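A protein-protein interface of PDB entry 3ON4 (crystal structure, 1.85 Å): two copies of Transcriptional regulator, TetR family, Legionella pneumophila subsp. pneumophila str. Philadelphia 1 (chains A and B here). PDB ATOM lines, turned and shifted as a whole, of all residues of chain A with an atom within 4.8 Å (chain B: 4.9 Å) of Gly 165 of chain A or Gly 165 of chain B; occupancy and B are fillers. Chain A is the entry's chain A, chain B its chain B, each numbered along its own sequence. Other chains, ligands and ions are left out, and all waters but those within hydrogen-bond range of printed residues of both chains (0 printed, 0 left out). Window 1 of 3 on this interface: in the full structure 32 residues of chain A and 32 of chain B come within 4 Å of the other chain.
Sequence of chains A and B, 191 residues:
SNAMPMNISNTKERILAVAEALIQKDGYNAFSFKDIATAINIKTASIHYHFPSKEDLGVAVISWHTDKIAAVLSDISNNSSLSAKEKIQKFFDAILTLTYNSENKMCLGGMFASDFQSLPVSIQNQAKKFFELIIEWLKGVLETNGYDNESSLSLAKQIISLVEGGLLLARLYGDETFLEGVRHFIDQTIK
Among the printed residues, pairs that only touch across the chains: Ser 161 of chain A with Gly 165 of chain B, Gly 165 of chain A with Ser 161 of chain B, Ser 161 of chain A with Gly 166 of chain B, Leu 162 of chain A with Ser 161 of chain B, Gly 166 of chain A with Ser 161 of chain B, Ser 161 of chain A with Leu 162 of chain B, Leu 169 of chain A with Ile 160 of chain B, Ser 161 of chain A with Ser 161 of chain B, Leu 162 of chain A with Leu 162 of chain B, Gly 165 of chain A with Gly 165 of chain B and Ser 161 of chain A with Leu 169 of chain B.
Of chain B, only Ser 161 and Gly 165 come within 4 Å of Gly 165 of chain A.
Of the printed residues of chain A, Leu 169 of chain B touches Ser 161 (3.9 Å).
Of the printed residues of chain B, Gly 166 of chain A touches Ser 161 (3.7 Å).
Printed residues of chain A within 4 Å of Ser 161 of chain B: Ser 161 (3.8 Å), Leu 162 (3.7 Å), Gly 165 (3.2 Å) and Gly 166 (3.7 Å).
Of the printed residues of chain A, Gly 166 of chain B touches Ser 161.
Leu 168 of chain A touches none of the printed residues of chain B.
Printed residues of chain A that touch a printed residue of chain B: Ser 161, Leu 162, Gly 165, Gly 166 and Leu 169.
Of the 10 printed residues of chain B, 6 touch a printed residue of chain A.
Hydrophobic or aromatic side chains of chain B within 4 Å of the printed part of chain A: Ile 160, Leu 162 and Leu 169.
Among the printed residues, no Asp or Glu carboxylate lies within 4 Å of a Lys or Arg side-chain nitrogen of the other chain.
Ser 161 of chain A touches its own counterpart, Ser 161 of chain B.
Ser 161 of chain A touches Leu 162 of chain B, and with the chains exchanged Leu 162 of chain A touches Ser 161 of chain B.
Ser 161 of chain A touches Gly 166 of chain B, and with the chains exchanged Gly 166 of chain A touches Ser 161 of chain B.
Leu 162 of chain A touches its own counterpart, Leu 162 of chain B.
Positions printed for both chains: 161, 162, 163, 164, 165, 166, 167, 168 and 169.
Of the 11 pairs that touch across the chains among the printed residues, 9 have their exchanged pair printed and touching as well.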
ATOM      1  N   SER A 161     -20.406   2.317  28.195  1.00  0.00           N
ATOM      2  CA  SER A 161     -21.073   1.875  26.965  1.00  0.00           C
ATOM      3  C   SER A 161     -21.459   3.082  26.111  1.00  0.00           C
ATOM      4  O   SER A 161     -21.236   3.099  24.889  1.00  0.00           O
ATOM      5  CB  SER A 161     -22.316   1.045  27.284  1.00  0.00           C
ATOM      6  OG  SER A 161     -21.961  -0.096  28.051  1.00  0.00           O
ATOM      7  N   LEU A 162     -22.012   4.109  26.756  1.00  0.00           N
ATOM      8  CA  LEU A 162     -22.475   5.274  26.035  1.00  0.00           C
ATOM      9  C   LEU A 162     -21.291   6.048  25.464  1.00  0.00           C
ATOM     10  O   LEU A 162     -21.362   6.527  24.344  1.00  0.00           O
ATOM     11  CB  LEU A 162     -23.312   6.166  26.936  1.00  0.00           C
ATOM     12  CG  LEU A 162     -24.121   7.301  26.342  1.00  0.00           C
ATOM     13  CD1 LEU A 162     -24.933   6.881  25.088  1.00  0.00           C
ATOM     14  CD2 LEU A 162     -25.056   7.821  27.427  1.00  0.00           C
ATOM     15  N   VAL A 163     -20.221   6.158  26.235  1.00  0.00           N
ATOM     16  CA  VAL A 163     -19.010   6.830  25.779  1.00  0.00           C
ATOM     17  C   VAL A 163     -18.478   6.127  24.529  1.00  0.00           C
ATOM     18  O   VAL A 163     -18.188   6.782  23.518  1.00  0.00           O
ATOM     19  CB  VAL A 163     -17.927   6.867  26.876  1.00  0.00           C
ATOM     20  CG1 VAL A 163     -16.526   7.192  26.277  1.00  0.00           C
ATOM     21  CG2 VAL A 163     -18.317   7.841  27.991  1.00  0.00           C
ATOM     22  N   GLU A 164     -18.356   4.800  24.582  1.00  0.00           N
ATOM     23  CA  GLU A 164     -17.806   4.040  23.458  1.00  0.00           C
ATOM     24  C   GLU A 164     -18.698   4.167  22.214  1.00  0.00           C
ATOM     25  O   GLU A 164     -18.229   4.486  21.111  1.00  0.00           O
ATOM     26  CB  GLU A 164     -17.566   2.579  23.830  1.00  0.00           C
ATOM     27  CG  GLU A 164     -16.485   2.372  24.907  1.00  0.00           C
ATOM     28  CD  GLU A 164     -15.104   2.804  24.487  1.00  0.00           C
ATOM     29  OE1 GLU A 164     -14.809   2.793  23.280  1.00  0.00           O
ATOM     30  OE2 GLU A 164     -14.271   3.119  25.369  1.00  0.00           O
ATOM     31  N   GLY A 165     -19.990   3.945  22.384  1.00  0.00           N
ATOM     32  CA  GLY A 165     -20.918   4.014  21.259  1.00  0.00           C
ATOM     33  C   GLY A 165     -21.049   5.424  20.698  1.00  0.00           C
ATOM     34  O   GLY A 165     -21.151   5.607  19.477  1.00  0.00           O
ATOM     35  N   GLY A 166     -21.067   6.419  21.579  1.00  0.00           N
ATOM     36  CA  GLY A 166     -21.109   7.825  21.176  1.00  0.00           C
ATOM     37  C   GLY A 166     -19.907   8.254  20.351  1.00  0.00           C
ATOM     38  O   GLY A 166     -20.049   8.940  19.312  1.00  0.00           O
ATOM     39  N   LEU A 167     -18.725   7.824  20.789  1.00  0.00           N
ATOM     40  CA  LEU A 167     -17.487   8.120  20.031  1.00  0.00           C
ATOM     41  C   LEU A 167     -17.495   7.415  18.699  1.00  0.00           C
ATOM     42  O   LEU A 167     -17.128   7.986  17.695  1.00  0.00           O
ATOM     43  CB  LEU A 167     -16.230   7.713  20.815  1.00  0.00           C
ATOM     44  CG  LEU A 167     -15.811   8.577  21.982  1.00  0.00           C
ATOM     45  CD1 LEU A 167     -14.657   7.931  22.772  1.00  0.00           C
ATOM     46  CD2 LEU A 167     -15.404   9.970  21.468  1.00  0.00           C
ATOM     47  N   LEU A 168     -17.933   6.165  18.692  1.00  0.00           N
ATOM     48  CA  LEU A 168     -17.974   5.350  17.482  1.00  0.00           C
ATOM     49  C   LEU A 168     -18.788   6.037  16.387  1.00  0.00           C
ATOM     50  O   LEU A 168     -18.361   6.134  15.224  1.00  0.00           O
ATOM     51  CB  LEU A 168     -18.604   3.999  17.829  1.00  0.00           C
ATOM     52  CG  LEU A 168     -18.527   2.859  16.843  1.00  0.00           C
ATOM     53  CD1 LEU A 168     -17.065   2.344  16.681  1.00  0.00           C
ATOM     54  CD2 LEU A 168     -19.435   1.710  17.342  1.00  0.00           C
ATOM     55  N   LEU A 169     -19.961   6.549  16.763  1.00  0.00           N
ATOM     56  CA  LEU A 169     -20.852   7.145  15.795  1.00  0.00           C
ATOM     57  C   LEU A 169     -20.501   8.612  15.505  1.00  0.00           C
ATOM     58  O   LEU A 169     -20.667   9.051  14.363  1.00  0.00           O
ATOM     59  CB  LEU A 169     -22.319   7.003  16.239  1.00  0.00           C
ATOM     60  CG  LEU A 169     -22.735   5.545  16.439  1.00  0.00           C
ATOM     61  CD1 LEU A 169     -24.172   5.453  16.887  1.00  0.00           C
ATOM     62  CD2 LEU A 169     -22.510   4.754  15.151  1.00  0.00           C
ATOM     63  N   ILE B 160     -29.099   4.350  20.194  1.00  0.00           N
ATOM     64  CA  ILE B 160     -28.210   3.553  19.305  1.00  0.00           C
ATOM     65  C   ILE B 160     -26.769   3.633  19.790  1.00  0.00           C
ATOM     66  O   ILE B 160     -26.062   2.644  19.729  1.00  0.00           O
ATOM     67  CB  ILE B 160     -28.352   3.910  17.805  1.00  0.00           C
ATOM     68  CG1 ILE B 160     -27.567   2.932  16.905  1.00  0.00           C
ATOM     69  CG2 ILE B 160     -27.906   5.354  17.535  1.00  0.00           C
ATOM     70  CD1 ILE B 160     -28.030   1.445  16.961  1.00  0.00           C
ATOM     71  N   SER B 161     -26.354   4.774  20.331  1.00  0.00           N
ATOM     72  CA  SER B 161     -25.019   4.867  20.939  1.00  0.00           C
ATOM     73  C   SER B 161     -24.884   3.829  22.074  1.00  0.00           C
ATOM     74  O   SER B 161     -23.888   3.099  22.152  1.00  0.00           O
ATOM     75  CB  SER B 161     -24.754   6.266  21.474  1.00  0.00           C
ATOM     76  OG  SER B 161     -24.722   7.238  20.439  1.00  0.00           O
ATOM     77  N   LEU B 162     -25.884   3.764  22.950  1.00  0.00           N
ATOM     78  CA  LEU B 162     -25.842   2.822  24.064  1.00  0.00           C
ATOM     79  C   LEU B 162     -25.923   1.373  23.595  1.00  0.00           C
ATOM     80  O   LEU B 162     -25.241   0.492  24.141  1.00  0.00           O
ATOM     81  CB  LEU B 162     -26.971   3.125  25.061  1.00  0.00           C
ATOM     82  CG  LEU B 162     -26.941   2.392  26.405  1.00  0.00           C
ATOM     83  CD1 LEU B 162     -25.662   2.630  27.192  1.00  0.00           C
ATOM     84  CD2 LEU B 162     -28.178   2.773  27.251  1.00  0.00           C
ATOM     85  N   VAL B 163     -26.760   1.112  22.594  1.00  0.00           N
ATOM     86  CA  VAL B 163     -26.850  -0.224  22.015  1.00  0.00           C
ATOM     87  C   VAL B 163     -25.489  -0.675  21.490  1.00  0.00           C
ATOM     88  O   VAL B 163     -25.027  -1.777  21.819  1.00  0.00           O
ATOM     89  CB  VAL B 163     -27.929  -0.318  20.907  1.00  0.00           C
ATOM     90  CG1 VAL B 163     -27.729  -1.585  20.043  1.00  0.00           C
ATOM     91  CG2 VAL B 163     -29.362  -0.271  21.512  1.00  0.00           C
ATOM     92  N   GLU B 164     -24.839   0.167  20.690  1.00  0.00           N
ATOM     93  CA  GLU B 164     -23.565  -0.179  20.087  1.00  0.00           C
ATOM     94  C   GLU B 164     -22.493  -0.403  21.139  1.00  0.00           C
ATOM     95  O   GLU B 164     -21.762  -1.401  21.094  1.00  0.00           O
ATOM     96  CB  GLU B 164     -23.111   0.860  19.065  1.00  0.00           C
ATOM     97  CG  GLU B 164     -23.983   0.963  17.817  1.00  0.00           C
ATOM     98  CD  GLU B 164     -24.013  -0.279  16.957  1.00  0.00           C
ATOM     99  OE1 GLU B 164     -22.984  -0.970  16.857  1.00  0.00           O
ATOM    100  OE2 GLU B 164     -25.080  -0.558  16.340  1.00  0.00           O
ATOM    101  N   GLY B 165     -22.403   0.506  22.096  1.00  0.00           N
ATOM    102  CA  GLY B 165     -21.422   0.368  23.171  1.00  0.00           C
ATOM    103  C   GLY B 165     -21.664  -0.830  24.084  1.00  0.00           C
ATOM    104  O   GLY B 165     -20.723  -1.500  24.496  1.00  0.00           O
ATOM    105  N   GLY B 166     -22.924  -1.099  24.402  1.00  0.00           N
ATOM    106  CA  GLY B 166     -23.320  -2.220  25.251  1.00  0.00           C
ATOM    107  C   GLY B 166     -22.975  -3.559  24.611  1.00  0.00           C
ATOM    108  O   GLY B 166     -22.440  -4.460  25.251  1.00  0.00           O
ATOM    109  N   LEU B 167     -23.265  -3.679  23.322  1.00  0.00           N
ATOM    110  CA  LEU B 167     -22.938  -4.868  22.571  1.00  0.00           C
ATOM    111  C   LEU B 167     -21.422  -5.055  22.474  1.00  0.00           C
ATOM    112  O   LEU B 167     -20.928  -6.152  22.622  1.00  0.00           O
ATOM    113  CB  LEU B 167     -23.542  -4.796  21.164  1.00  0.00           C
ATOM    114  CG  LEU B 167     -25.049  -4.936  21.077  1.00  0.00           C
ATOM    115  CD1 LEU B 167     -25.399  -4.672  19.633  1.00  0.00           C
ATOM    116  CD2 LEU B 167     -25.514  -6.330  21.569  1.00  0.00           C
ATOM    117  N   LEU B 168     -20.701  -3.974  22.241  1.00  0.00           N
ATOM    118  CA  LEU B 168     -19.262  -4.000  22.139  1.00  0.00           C
ATOM    119  C   LEU B 168     -18.579  -4.578  23.378  1.00  0.00           C
ATOM    120  O   LEU B 168     -17.664  -5.395  23.277  1.00  0.00           O
ATOM    121  CB  LEU B 168     -18.753  -2.567  21.908  1.00  0.00           C
ATOM    122  CG  LEU B 168     -17.286  -2.413  21.571  1.00  0.00           C
ATOM    123  CD1 LEU B 168     -17.005  -2.858  20.128  1.00  0.00           C
ATOM    124  CD2 LEU B 168     -16.877  -0.961  21.771  1.00  0.00           C
ATOM    125  N   LEU B 169     -19.023  -4.144  24.547  1.00  0.00           N
ATOM    126  CA  LEU B 169     -18.427  -4.562  25.797  1.00  0.00           C
ATOM    127  C   LEU B 169     -18.996  -5.870  26.332  1.00  0.00           C
ATOM    128  O   LEU B 169     -18.255  -6.648  26.943  1.00  0.00           O
ATOM    129  CB  LEU B 169     -18.540  -3.422  26.838  1.00  0.00           C
ATOM    130  CG  LEU B 169     -17.970  -2.072  26.364  1.00  0.00           C
ATOM    131  CD1 LEU B 169     -18.191  -0.976  27.388  1.00  0.00           C
ATOM    132  CD2 LEU B 169     -16.466  -2.193  25.972  1.00  0.00           C
